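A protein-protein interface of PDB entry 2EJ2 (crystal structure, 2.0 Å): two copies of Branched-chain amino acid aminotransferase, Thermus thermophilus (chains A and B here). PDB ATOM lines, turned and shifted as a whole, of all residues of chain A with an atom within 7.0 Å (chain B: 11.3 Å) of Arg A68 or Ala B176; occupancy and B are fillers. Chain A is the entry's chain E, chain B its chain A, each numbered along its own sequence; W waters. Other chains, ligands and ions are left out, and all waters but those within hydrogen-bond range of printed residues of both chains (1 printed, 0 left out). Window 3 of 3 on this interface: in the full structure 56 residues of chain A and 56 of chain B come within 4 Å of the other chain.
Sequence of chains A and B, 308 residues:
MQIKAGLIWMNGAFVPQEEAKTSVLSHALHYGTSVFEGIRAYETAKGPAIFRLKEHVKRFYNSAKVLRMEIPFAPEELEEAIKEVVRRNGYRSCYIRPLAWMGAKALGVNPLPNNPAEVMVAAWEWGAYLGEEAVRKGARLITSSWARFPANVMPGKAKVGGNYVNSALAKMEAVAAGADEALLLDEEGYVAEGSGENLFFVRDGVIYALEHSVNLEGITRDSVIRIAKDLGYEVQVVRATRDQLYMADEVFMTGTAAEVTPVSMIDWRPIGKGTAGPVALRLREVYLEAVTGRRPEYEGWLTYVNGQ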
ATOM      1  N   SER A  63     -16.423 -25.052  21.338  1.00  0.00           N
ATOM      2  CA  SER A  63     -16.457 -23.741  21.984  1.00  0.00           C
ATOM      3  C   SER A  63     -16.152 -22.625  20.981  1.00  0.00           C
ATOM      4  O   SER A  63     -16.781 -21.567  21.007  1.00  0.00           O
ATOM      5  CB  SER A  63     -15.453 -23.685  23.141  1.00  0.00           C
ATOM      6  OG  SER A  63     -15.860 -24.515  24.221  1.00  0.00           O
ATOM      7  N   ALA A  64     -15.182 -22.864  20.103  1.00  0.00           N
ATOM      8  CA  ALA A  64     -14.810 -21.876  19.095  1.00  0.00           C
ATOM      9  C   ALA A  64     -15.984 -21.623  18.149  1.00  0.00           C
ATOM     10  O   ALA A  64     -16.230 -20.491  17.737  1.00  0.00           O
ATOM     11  CB  ALA A  64     -13.586 -22.362  18.301  1.00  0.00           C
ATOM     12  N   LYS A  65     -16.705 -22.687  17.810  1.00  0.00           N
ATOM     13  CA  LYS A  65     -17.847 -22.573  16.911  1.00  0.00           C
ATOM     14  C   LYS A  65     -18.873 -21.593  17.473  1.00  0.00           C
ATOM     15  O   LYS A  65     -19.495 -20.841  16.726  1.00  0.00           O
ATOM     16  CB  LYS A  65     -18.496 -23.940  16.715  1.00  0.00           C
ATOM     17  CG  LYS A  65     -19.548 -23.984  15.621  1.00  0.00           C
ATOM     18  CD  LYS A  65     -20.247 -25.337  15.597  1.00  0.00           C
ATOM     19  CE  LYS A  65     -19.249 -26.477  15.445  1.00  0.00           C
ATOM     20  NZ  LYS A  65     -19.888 -27.811  15.619  1.00  0.00           N
ATOM     21  N   VAL A  66     -19.042 -21.603  18.789  1.00  0.00           N
ATOM     22  CA  VAL A  66     -19.995 -20.712  19.438  1.00  0.00           C
ATOM     23  C   VAL A  66     -19.660 -19.240  19.198  1.00  0.00           C
ATOM     24  O   VAL A  66     -20.558 -18.408  19.077  1.00  0.00           O
ATOM     25  CB  VAL A  66     -20.060 -20.988  20.955  1.00  0.00           C
ATOM     26  CG1 VAL A  66     -20.873 -19.916  21.646  1.00  0.00           C
ATOM     27  CG2 VAL A  66     -20.684 -22.357  21.200  1.00  0.00           C
ATOM     28  N   LEU A  67     -18.368 -18.918  19.141  1.00  0.00           N
ATOM     29  CA  LEU A  67     -17.936 -17.542  18.897  1.00  0.00           C
ATOM     30  C   LEU A  67     -17.680 -17.307  17.411  1.00  0.00           C
ATOM     31  O   LEU A  67     -17.209 -16.241  17.027  1.00  0.00           O
ATOM     32  CB  LEU A  67     -16.642 -17.232  19.653  1.00  0.00           C
ATOM     33  CG  LEU A  67     -16.643 -17.025  21.165  1.00  0.00           C
ATOM     34  CD1 LEU A  67     -15.228 -16.688  21.608  1.00  0.00           C
ATOM     35  CD2 LEU A  67     -17.594 -15.895  21.545  1.00  0.00           C
ATOM     36  N   ARG A  68     -17.985 -18.302  16.584  1.00  0.00           N
ATOM     37  CA  ARG A  68     -17.744 -18.209  15.146  1.00  0.00           C
ATOM     38  C   ARG A  68     -16.251 -17.964  14.954  1.00  0.00           C
ATOM     39  O   ARG A  68     -15.815 -17.287  14.022  1.00  0.00           O
ATOM     40  CB  ARG A  68     -18.570 -17.073  14.525  1.00  0.00           C
ATOM     41  CG  ARG A  68     -20.079 -17.287  14.648  1.00  0.00           C
ATOM     42  CD  ARG A  68     -20.863 -16.241  13.872  1.00  0.00           C
ATOM     43  NE  ARG A  68     -20.628 -16.343  12.436  1.00  0.00           N
ATOM     44  CZ  ARG A  68     -21.110 -15.494  11.536  1.00  0.00           C
ATOM     45  NH1 ARG A  68     -21.859 -14.468  11.922  1.00  0.00           N
ATOM     46  NH2 ARG A  68     -20.841 -15.670  10.249  1.00  0.00           N
ATOM     47  N   MET A  69     -15.473 -18.528  15.870  1.00  0.00           N
ATOM     48  CA  MET A  69     -14.025 -18.410  15.853  1.00  0.00           C
ATOM     49  C   MET A  69     -13.450 -19.537  15.000  1.00  0.00           C
ATOM     50  O   MET A  69     -13.893 -20.680  15.101  1.00  0.00           O
ATOM     51  CB  MET A  69     -13.489 -18.515  17.281  1.00  0.00           C
ATOM     52  CG  MET A  69     -11.981 -18.628  17.384  1.00  0.00           C
ATOM     53  SD  MET A  69     -11.478 -19.080  19.048  1.00  0.00           S
ATOM     54  CE  MET A  69     -11.430 -17.486  19.837  1.00  0.00           C
ATOM     55  N   GLU A  70     -12.470 -19.210  14.162  1.00  0.00           N
ATOM     56  CA  GLU A  70     -11.834 -20.195  13.290  1.00  0.00           C
ATOM     57  C   GLU A  70     -10.489 -20.655  13.845  1.00  0.00           C
ATOM     58  O   GLU A  70      -9.593 -19.843  14.063  1.00  0.00           O
ATOM     59  CB  GLU A  70     -11.613 -19.604  11.893  1.00  0.00           C
ATOM     60  CG  GLU A  70     -12.878 -19.220  11.147  1.00  0.00           C
ATOM     61  CD  GLU A  70     -13.788 -20.407  10.889  1.00  0.00           C
ATOM     62  OE1 GLU A  70     -13.269 -21.481  10.511  1.00  0.00           O
ATOM     63  OE2 GLU A  70     -15.022 -20.261  11.053  1.00  0.00           O
ATOM     64  N   MET A 102      -8.727 -14.401  19.940  1.00  0.00           N
ATOM     65  CA  MET A 102      -8.781 -13.445  18.842  1.00  0.00           C
ATOM     66  C   MET A 102      -7.629 -12.470  19.027  1.00  0.00           C
ATOM     67  O   MET A 102      -7.431 -11.936  20.121  1.00  0.00           O
ATOM     68  CB  MET A 102     -10.123 -12.708  18.844  1.00  0.00           C
ATOM     69  CG  MET A 102     -11.325 -13.625  18.643  1.00  0.00           C
ATOM     70  SD  MET A 102     -11.121 -14.784  17.259  1.00  0.00           S
ATOM     71  CE  MET A 102     -11.253 -13.703  15.875  1.00  0.00           C
ATOM     72  N   ASN A 110     -16.911  -6.608  17.206  1.00  0.00           N
ATOM     73  CA  ASN A 110     -17.175  -7.765  16.351  1.00  0.00           C
ATOM     74  C   ASN A 110     -15.825  -8.461  16.163  1.00  0.00           C
ATOM     75  O   ASN A 110     -14.867  -7.841  15.698  1.00  0.00           O
ATOM     76  CB  ASN A 110     -17.713  -7.305  14.990  1.00  0.00           C
ATOM     77  CG  ASN A 110     -18.106  -8.461  14.095  1.00  0.00           C
ATOM     78  OD1 ASN A 110     -17.720  -9.606  14.332  1.00  0.00           O
ATOM     79  ND2 ASN A 110     -18.870  -8.165  13.046  1.00  0.00           N
ATOM     80  N   PRO A 111     -15.727  -9.754  16.517  1.00  0.00           N
ATOM     81  CA  PRO A 111     -14.455 -10.471  16.366  1.00  0.00           C
ATOM     82  C   PRO A 111     -14.199 -11.120  15.000  1.00  0.00           C
ATOM     83  O   PRO A 111     -13.080 -11.546  14.718  1.00  0.00           O
ATOM     84  CB  PRO A 111     -14.527 -11.509  17.475  1.00  0.00           C
ATOM     85  CG  PRO A 111     -15.969 -11.904  17.422  1.00  0.00           C
ATOM     86  CD  PRO A 111     -16.690 -10.563  17.286  1.00  0.00           C
ATOM     87  N   LEU A 112     -15.223 -11.204  14.160  1.00  0.00           N
ATOM     88  CA  LEU A 112     -15.070 -11.830  12.845  1.00  0.00           C
ATOM     89  C   LEU A 112     -13.897 -11.289  12.028  1.00  0.00           C
ATOM     90  O   LEU A 112     -13.202 -12.055  11.359  1.00  0.00           O
ATOM     91  CB  LEU A 112     -16.368 -11.710  12.045  1.00  0.00           C
ATOM     92  CG  LEU A 112     -17.510 -12.607  12.534  1.00  0.00           C
ATOM     93  CD1 LEU A 112     -18.786 -12.293  11.769  1.00  0.00           C
ATOM     94  CD2 LEU A 112     -17.122 -14.071  12.349  1.00  0.00           C
ATOM     95  N   ASN A 115     -10.400 -13.129  12.664  1.00  0.00           N
ATOM     96  CA  ASN A 115     -10.096 -14.520  12.327  1.00  0.00           C
ATOM     97  C   ASN A 115      -8.944 -14.597  11.328  1.00  0.00           C
ATOM     98  O   ASN A 115      -8.727 -13.669  10.548  1.00  0.00           O
ATOM     99  CB  ASN A 115     -11.324 -15.220  11.737  1.00  0.00           C
ATOM    100  CG  ASN A 115     -12.230 -15.793  12.802  1.00  0.00           C
ATOM    101  OD1 ASN A 115     -11.775 -16.514  13.687  1.00  0.00           O
ATOM    102  ND2 ASN A 115     -13.521 -15.486  12.721  1.00  0.00           N
ATOM    103  N   ARG B 140     -29.372   1.517  11.049  1.00  0.00           N
ATOM    104  CA  ARG B 140     -30.429   0.516  11.042  1.00  0.00           C
ATOM    105  C   ARG B 140     -30.083  -0.507  12.117  1.00  0.00           C
ATOM    106  O   ARG B 140     -28.988  -1.076  12.111  1.00  0.00           O
ATOM    107  CB  ARG B 140     -30.515  -0.186   9.681  1.00  0.00           C
ATOM    108  CG  ARG B 140     -30.844   0.722   8.511  1.00  0.00           C
ATOM    109  CD  ARG B 140     -31.145  -0.099   7.263  1.00  0.00           C
ATOM    110  NE  ARG B 140     -30.122  -1.116   7.021  1.00  0.00           N
ATOM    111  CZ  ARG B 140     -28.849  -0.851   6.728  1.00  0.00           C
ATOM    112  NH1 ARG B 140     -28.431   0.406   6.633  1.00  0.00           N
ATOM    113  NH2 ARG B 140     -27.989  -1.844   6.542  1.00  0.00           N
ATOM    114  N   LEU B 141     -31.003  -0.730  13.048  1.00  0.00           N
ATOM    115  CA  LEU B 141     -30.763  -1.690  14.116  1.00  0.00           C
ATOM    116  C   LEU B 141     -31.673  -2.901  13.997  1.00  0.00           C
ATOM    117  O   LEU B 141     -32.691  -2.874  13.305  1.00  0.00           O
ATOM    118  CB  LEU B 141     -31.009  -1.055  15.493  1.00  0.00           C
ATOM    119  CG  LEU B 141     -30.325   0.248  15.903  1.00  0.00           C
ATOM    120  CD1 LEU B 141     -30.717   0.591  17.329  1.00  0.00           C
ATOM    121  CD2 LEU B 141     -28.829   0.115  15.780  1.00  0.00           C
ATOM    122  N   ILE B 142     -31.286  -3.965  14.682  1.00  0.00           N
ATOM    123  CA  ILE B 142     -32.069  -5.183  14.739  1.00  0.00           C
ATOM    124  C   ILE B 142     -31.976  -5.638  16.187  1.00  0.00           C
ATOM    125  O   ILE B 142     -30.912  -5.551  16.800  1.00  0.00           O
ATOM    126  CB  ILE B 142     -31.515  -6.269  13.800  1.00  0.00           C
ATOM    127  CG1 ILE B 142     -31.908  -5.939  12.355  1.00  0.00           C
ATOM    128  CG2 ILE B 142     -32.066  -7.627  14.192  1.00  0.00           C
ATOM    129  CD1 ILE B 142     -31.372  -6.911  11.323  1.00  0.00           C
ATOM    130  N   THR B 143     -33.090  -6.090  16.750  1.00  0.00           N
ATOM    131  CA  THR B 143     -33.073  -6.543  18.133  1.00  0.00           C
ATOM    132  C   THR B 143     -32.389  -7.905  18.200  1.00  0.00           C
ATOM    133  O   THR B 143     -32.703  -8.814  17.432  1.00  0.00           O
ATOM    134  CB  THR B 143     -34.497  -6.621  18.709  1.00  0.00           C
ATOM    135  OG1 THR B 143     -35.130  -5.339  18.576  1.00  0.00           O
ATOM    136  CG2 THR B 143     -34.454  -7.006  20.182  1.00  0.00           C
ATOM    137  N   SER B 144     -31.438  -8.033  19.120  1.00  0.00           N
ATOM    138  CA  SER B 144     -30.666  -9.260  19.286  1.00  0.00           C
ATOM    139  C   SER B 144     -31.388 -10.410  19.985  1.00  0.00           C
ATOM    140  O   SER B 144     -32.324 -10.201  20.768  1.00  0.00           O
ATOM    141  CB  SER B 144     -29.376  -8.950  20.048  1.00  0.00           C
ATOM    142  OG  SER B 144     -28.604 -10.125  20.242  1.00  0.00           O
ATOM    143  N   SER B 145     -30.935 -11.626  19.689  1.00  0.00           N
ATOM    144  CA  SER B 145     -31.484 -12.831  20.300  1.00  0.00           C
ATOM    145  C   SER B 145     -30.683 -13.098  21.574  1.00  0.00           C
ATOM    146  O   SER B 145     -30.924 -14.070  22.293  1.00  0.00           O
ATOM    147  CB  SER B 145     -31.369 -14.021  19.349  1.00  0.00           C
ATOM    148  OG  SER B 145     -30.016 -14.308  19.051  1.00  0.00           O
ATOM    149  N   TRP B 146     -29.700 -12.242  21.832  1.00  0.00           N
ATOM    150  CA  TRP B 146     -28.907 -12.359  23.046  1.00  0.00           C
ATOM    151  C   TRP B 146     -29.382 -11.246  23.977  1.00  0.00           C
ATOM    152  O   TRP B 146     -29.456 -10.088  23.579  1.00  0.00           O
ATOM    153  CB  TRP B 146     -27.412 -12.197  22.751  1.00  0.00           C
ATOM    154  CG  TRP B 146     -26.844 -13.328  21.948  1.00  0.00           C
ATOM    155  CD1 TRP B 146     -26.746 -13.401  20.589  1.00  0.00           C
ATOM    156  CD2 TRP B 146     -26.339 -14.571  22.455  1.00  0.00           C
ATOM    157  NE1 TRP B 146     -26.212 -14.615  20.214  1.00  0.00           N
ATOM    158  CE2 TRP B 146     -25.955 -15.352  21.340  1.00  0.00           C
ATOM    159  CE3 TRP B 146     -26.176 -15.103  23.743  1.00  0.00           C
ATOM    160  CZ2 TRP B 146     -25.416 -16.641  21.474  1.00  0.00           C
ATOM    161  CZ3 TRP B 146     -25.639 -16.386  23.877  1.00  0.00           C
ATOM    162  CH2 TRP B 146     -25.267 -17.139  22.746  1.00  0.00           C
ATOM    163  N   VAL B 165     -18.331 -10.271  25.585  1.00  0.00           N
ATOM    164  CA  VAL B 165     -18.583 -11.478  24.817  1.00  0.00           C
ATOM    165  C   VAL B 165     -20.061 -11.349  24.428  1.00  0.00           C
ATOM    166  O   VAL B 165     -20.456 -11.655  23.301  1.00  0.00           O
ATOM    167  CB  VAL B 165     -18.378 -12.756  25.668  1.00  0.00           C
ATOM    168  CG1 VAL B 165     -19.080 -13.944  25.006  1.00  0.00           C
ATOM    169  CG2 VAL B 165     -16.879 -13.049  25.815  1.00  0.00           C
ATOM    170  N   SER B 167     -21.694  -8.561  24.123  1.00  0.00           N
ATOM    171  CA  SER B 167     -21.762  -7.520  23.102  1.00  0.00           C
ATOM    172  C   SER B 167     -21.290  -8.039  21.741  1.00  0.00           C
ATOM    173  O   SER B 167     -21.889  -7.729  20.711  1.00  0.00           O
ATOM    174  CB  SER B 167     -20.906  -6.315  23.499  1.00  0.00           C
ATOM    175  OG  SER B 167     -21.502  -5.578  24.550  1.00  0.00           O
ATOM    176  N   ALA B 168     -20.215  -8.825  21.742  1.00  0.00           N
ATOM    177  CA  ALA B 168     -19.665  -9.368  20.497  1.00  0.00           C
ATOM    178  C   ALA B 168     -20.663 -10.292  19.802  1.00  0.00           C
ATOM    179  O   ALA B 168     -20.863 -10.213  18.586  1.00  0.00           O
ATOM    180  CB  ALA B 168     -18.363 -10.124  20.784  1.00  0.00           C
ATOM    181  N   LEU B 169     -21.285 -11.175  20.577  1.00  0.00           N
ATOM    182  CA  LEU B 169     -22.265 -12.102  20.028  1.00  0.00           C
ATOM    183  C   LEU B 169     -23.440 -11.355  19.387  1.00  0.00           C
ATOM    184  O   LEU B 169     -23.923 -11.744  18.326  1.00  0.00           O
ATOM    185  CB  LEU B 169     -22.766 -13.043  21.133  1.00  0.00           C
ATOM    186  CG  LEU B 169     -21.760 -14.103  21.603  1.00  0.00           C
ATOM    187  CD1 LEU B 169     -22.256 -14.793  22.876  1.00  0.00           C
ATOM    188  CD2 LEU B 169     -21.561 -15.132  20.484  1.00  0.00           C
ATOM    189  N   ALA B 170     -23.891 -10.279  20.026  1.00  0.00           N
ATOM    190  CA  ALA B 170     -25.008  -9.498  19.500  1.00  0.00           C
ATOM    191  C   ALA B 170     -24.611  -8.716  18.246  1.00  0.00           C
ATOM    192  O   ALA B 170     -25.363  -8.660  17.274  1.00  0.00           O
ATOM    193  CB  ALA B 170     -25.527  -8.537  20.568  1.00  0.00           C
ATOM    194  N   LYS B 171     -23.425  -8.117  18.268  1.00  0.00           N
ATOM    195  CA  LYS B 171     -22.954  -7.338  17.123  1.00  0.00           C
ATOM    196  C   LYS B 171     -22.815  -8.224  15.885  1.00  0.00           C
ATOM    197  O   LYS B 171     -23.276  -7.855  14.803  1.00  0.00           O
ATOM    198  CB  LYS B 171     -21.616  -6.662  17.457  1.00  0.00           C
ATOM    199  CG  LYS B 171     -21.085  -5.705  16.384  1.00  0.00           C
ATOM    200  CD  LYS B 171     -22.088  -4.605  16.064  1.00  0.00           C
ATOM    201  CE  LYS B 171     -21.557  -3.644  15.015  1.00  0.00           C
ATOM    202  NZ  LYS B 171     -20.368  -2.899  15.518  1.00  0.00           N
ATOM    203  N   MET B 172     -22.197  -9.392  16.036  1.00  0.00           N
ATOM    204  CA  MET B 172     -22.036 -10.299  14.898  1.00  0.00           C
ATOM    205  C   MET B 172     -23.389 -10.653  14.311  1.00  0.00           C
ATOM    206  O   MET B 172     -23.554 -10.712  13.094  1.00  0.00           O
ATOM    207  CB  MET B 172     -21.332 -11.592  15.312  1.00  0.00           C
ATOM    208  CG  MET B 172     -19.865 -11.435  15.634  1.00  0.00           C
ATOM    209  SD  MET B 172     -19.046 -13.038  15.701  1.00  0.00           S
ATOM    210  CE  MET B 172     -19.629 -13.646  17.302  1.00  0.00           C
ATOM    211  N   GLU B 173     -24.356 -10.894  15.191  1.00  0.00           N
ATOM    212  CA  GLU B 173     -25.704 -11.245  14.771  1.00  0.00           C
ATOM    213  C   GLU B 173     -26.345 -10.123  13.955  1.00  0.00           C
ATOM    214  O   GLU B 173     -26.914 -10.368  12.894  1.00  0.00           O
ATOM    215  CB  GLU B 173     -26.568 -11.543  15.999  1.00  0.00           C
ATOM    216  CG  GLU B 173     -27.983 -11.977  15.668  1.00  0.00           C
ATOM    217  CD  GLU B 173     -28.844 -12.152  16.908  1.00  0.00           C
ATOM    218  OE1 GLU B 173     -29.810 -12.937  16.857  1.00  0.00           O
ATOM    219  OE2 GLU B 173     -28.562 -11.502  17.932  1.00  0.00           O
ATOM    220  N   ALA B 174     -26.256  -8.894  14.454  1.00  0.00           N
ATOM    221  CA  ALA B 174     -26.835  -7.750  13.759  1.00  0.00           C
ATOM    222  C   ALA B 174     -26.213  -7.595  12.374  1.00  0.00           C
ATOM    223  O   ALA B 174     -26.924  -7.520  11.370  1.00  0.00           O
ATOM    224  CB  ALA B 174     -26.625  -6.475  14.576  1.00  0.00           C
ATOM    225  N   VAL B 175     -24.887  -7.557  12.323  1.00  0.00           N
ATOM    226  CA  VAL B 175     -24.181  -7.413  11.054  1.00  0.00           C
ATOM    227  C   VAL B 175     -24.537  -8.550  10.096  1.00  0.00           C
ATOM    228  O   VAL B 175     -24.771  -8.320   8.908  1.00  0.00           O
ATOM    229  CB  VAL B 175     -22.644  -7.376  11.269  1.00  0.00           C
ATOM    230  CG1 VAL B 175     -21.927  -7.271   9.926  1.00  0.00           C
ATOM    231  CG2 VAL B 175     -22.274  -6.186  12.148  1.00  0.00           C
ATOM    232  N   ALA B 176     -24.594  -9.774  10.611  1.00  0.00           N
ATOM    233  CA  ALA B 176     -24.930 -10.920   9.772  1.00  0.00           C
ATOM    234  C   ALA B 176     -26.352 -10.783   9.244  1.00  0.00           C
ATOM    235  O   ALA B 176     -26.673 -11.274   8.161  1.00  0.00           O
ATOM    236  CB  ALA B 176     -24.790 -12.212  10.559  1.00  0.00           C
ATOM    237  N   ALA B 177     -27.200 -10.106  10.012  1.00  0.00           N
ATOM    238  CA  ALA B 177     -28.592  -9.902   9.620  1.00  0.00           C
ATOM    239  C   ALA B 177     -28.753  -8.711   8.671  1.00  0.00           C
ATOM    240  O   ALA B 177     -29.856  -8.425   8.216  1.00  0.00           O
ATOM    241  CB  ALA B 177     -29.460  -9.706  10.863  1.00  0.00           C
ATOM    242  N   GLY B 178     -27.652  -8.017   8.387  1.00  0.00           N
ATOM    243  CA  GLY B 178     -27.698  -6.879   7.481  1.00  0.00           C
ATOM    244  C   GLY B 178     -27.862  -5.523   8.142  1.00  0.00           C
ATOM    245  O   GLY B 178     -28.033  -4.512   7.458  1.00  0.00           O
ATOM    246  N   ALA B 179     -27.798  -5.492   9.471  1.00  0.00           N
ATOM    247  CA  ALA B 179     -27.955  -4.249  10.217  1.00  0.00           C
ATOM    248  C   ALA B 179     -26.616  -3.600  10.553  1.00  0.00           C
ATOM    249  O   ALA B 179     -25.563  -4.201  10.364  1.00  0.00           O
ATOM    250  CB  ALA B 179     -28.744  -4.508  11.504  1.00  0.00           C
ATOM    251  N   ASP B 180     -26.669  -2.370  11.053  1.00  0.00           N
ATOM    252  CA  ASP B 180     -25.464  -1.639  11.429  1.00  0.00           C
ATOM    253  C   ASP B 180     -25.084  -1.912  12.874  1.00  0.00           C
ATOM    254  O   ASP B 180     -23.907  -1.923  13.227  1.00  0.00           O
ATOM    255  CB  ASP B 180     -25.675  -0.133  11.276  1.00  0.00           C
ATOM    256  CG  ASP B 180     -25.943   0.277   9.846  1.00  0.00           C
ATOM    257  OD1 ASP B 180     -25.107  -0.047   8.979  1.00  0.00           O
ATOM    258  OD2 ASP B 180     -26.987   0.920   9.594  1.00  0.00           O
ATOM    259  N   GLU B 181     -26.087  -2.126  13.713  1.00  0.00           N
ATOM    260  CA  GLU B 181     -25.833  -2.345  15.125  1.00  0.00           C
ATOM    261  C   GLU B 181     -26.924  -3.197  15.750  1.00  0.00           C
ATOM    262  O   GLU B 181     -28.012  -3.337  15.192  1.00  0.00           O
ATOM    263  CB  GLU B 181     -25.755  -0.987  15.835  1.00  0.00           C
ATOM    264  CG  GLU B 181     -25.526  -1.075  17.328  1.00  0.00           C
ATOM    265  CD  GLU B 181     -24.203  -1.732  17.663  1.00  0.00           C
ATOM    266  OE1 GLU B 181     -23.159  -1.067  17.506  1.00  0.00           O
ATOM    267  OE2 GLU B 181     -24.212  -2.915  18.070  1.00  0.00           O
ATOM    268  N   ALA B 182     -26.622  -3.774  16.907  1.00  0.00           N
ATOM    269  CA  ALA B 182     -27.586  -4.602  17.610  1.00  0.00           C
ATOM    270  C   ALA B 182     -28.200  -3.840  18.770  1.00  0.00           C
ATOM    271  O   ALA B 182     -27.537  -3.033  19.422  1.00  0.00           O
ATOM    272  CB  ALA B 182     -26.916  -5.870  18.134  1.00  0.00           C
ATOM    273  N   LEU B 183     -29.478  -4.105  19.007  1.00  0.00           N
ATOM    274  CA  LEU B 183     -30.220  -3.517  20.112  1.00  0.00           C
ATOM    275  C   LEU B 183     -30.521  -4.695  21.033  1.00  0.00           C
ATOM    276  O   LEU B 183     -31.191  -5.644  20.631  1.00  0.00           O
ATOM    277  CB  LEU B 183     -31.521  -2.893  19.598  1.00  0.00           C
ATOM    278  CG  LEU B 183     -32.656  -2.562  20.573  1.00  0.00           C
ATOM    279  CD1 LEU B 183     -32.109  -2.022  21.870  1.00  0.00           C
ATOM    280  CD2 LEU B 183     -33.588  -1.545  19.921  1.00  0.00           C
ATOM    281  N   TRP B 268     -36.404  -3.673  10.661  1.00  0.00           N
ATOM    282  CA  TRP B 268     -37.000  -3.379   9.359  1.00  0.00           C
ATOM    283  C   TRP B 268     -38.240  -2.499   9.412  1.00  0.00           C
ATOM    284  O   TRP B 268     -38.976  -2.387   8.431  1.00  0.00           O
ATOM    285  CB  TRP B 268     -37.311  -4.687   8.635  1.00  0.00           C
ATOM    286  CG  TRP B 268     -36.129  -5.600   8.613  1.00  0.00           C
ATOM    287  CD1 TRP B 268     -36.091  -6.892   9.036  1.00  0.00           C
ATOM    288  CD2 TRP B 268     -34.796  -5.275   8.190  1.00  0.00           C
ATOM    289  NE1 TRP B 268     -34.819  -7.397   8.907  1.00  0.00           N
ATOM    290  CE2 TRP B 268     -34.003  -6.425   8.391  1.00  0.00           C
ATOM    291  CE3 TRP B 268     -34.193  -4.121   7.666  1.00  0.00           C
ATOM    292  CZ2 TRP B 268     -32.634  -6.461   8.085  1.00  0.00           C
ATOM    293  CZ3 TRP B 268     -32.827  -4.154   7.362  1.00  0.00           C
ATOM    294  CH2 TRP B 268     -32.066  -5.320   7.575  1.00  0.00           C
HETATM  295  O   HOH W   1     -17.447  -3.854  15.437  1.00  0.00           O
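Of chain B, only Ala B176 (3.9 Å) comes within 4 Å of Arg A68. Printed residues of chain A within 4 Å of Ala B176: Arg A68 (3.9 Å). No residue of chain B comes within 4 Å of Ala A64. Of the printed residues of chain B, Val A66 touches Leu B169. Of chain B, only Met B172 (3.6 Å) comes within 4 Å of Leu A67. Of chain B, only Met B172 comes within 4 Å of Leu A112. Of the printed residues of chain A, Leu B169 touches Val A66 (3.7 Å). Of the printed residues of chain A, Ala B168 touches Pro A111 (3.9 Å). Of the printed residues of chain B, Pro A111 touches Ala B168 (3.9 Å) and Met B172 (3.7 Å). Of the printed residues of chain A, Met B172 touches Leu A67 (3.6 Å), Asn A110 (3.1 Å), Pro A111 (3.7 Å) and Leu A112 (3.5 Å). Of the printed residues of chain B, Asn A110 touches Lys B171 and Met B172. The nearest residue of chain A that does not touch Ala B176 is Leu A112 (6.1 Å). The nearest printed residue of chain A that does not touch Ala B168 is Asn A110 (5.0 Å).
Of the 26 printed residues of chain B, 5 touch a printed residue of chain A. Hydrophobic or aromatic side chains of chain B that line the printed part of chain A: Ala B168, Leu B169, Met B172 and Ala B176. Among the printed residues, 8 pairs touch across the chains. Among the printed residues, no Asp or Glu carboxylate lies within 4 Å of a Lys or Arg side-chain nitrogen of the other chain.
The side-chain amino group (NZ) of Lys B171 is in salt-bridge range of the side-chain carboxylate (OE1) of Glu B181, at 3.9 Å. O of Arg A68 lies within hydrogen-bond range of ND2 of Asn A115 (3.2 Å). N of Leu A112 lies within hydrogen-bond range of OD1 of Asn A110 (3.0 Å).
No position is printed for both chains. Of the 8 pairs that touch across the chains among the printed residues, none has its exchanged pair printed and touching as well.
Water W1 lies within hydrogen-bond range of NZ of Lys B171 (3.1 Å) and N of Asn A110 (3.3 Å).
Among the printed residues, merely in contact across the chains: Asn A110 with Met B172 (3.1 Å), Leu A112 with Met B172 (3.5 Å), Leu A67 with Met B172 (3.6 Å), Pro A111 with Met B172 (3.7 Å), Val A66 with Leu B169 (3.7 Å), Pro A111 with Ala B168 (3.9 Å), Arg A68 with Ala B176 (3.9 Å) and Asn A110 with Lys B171 (3.98 Å).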
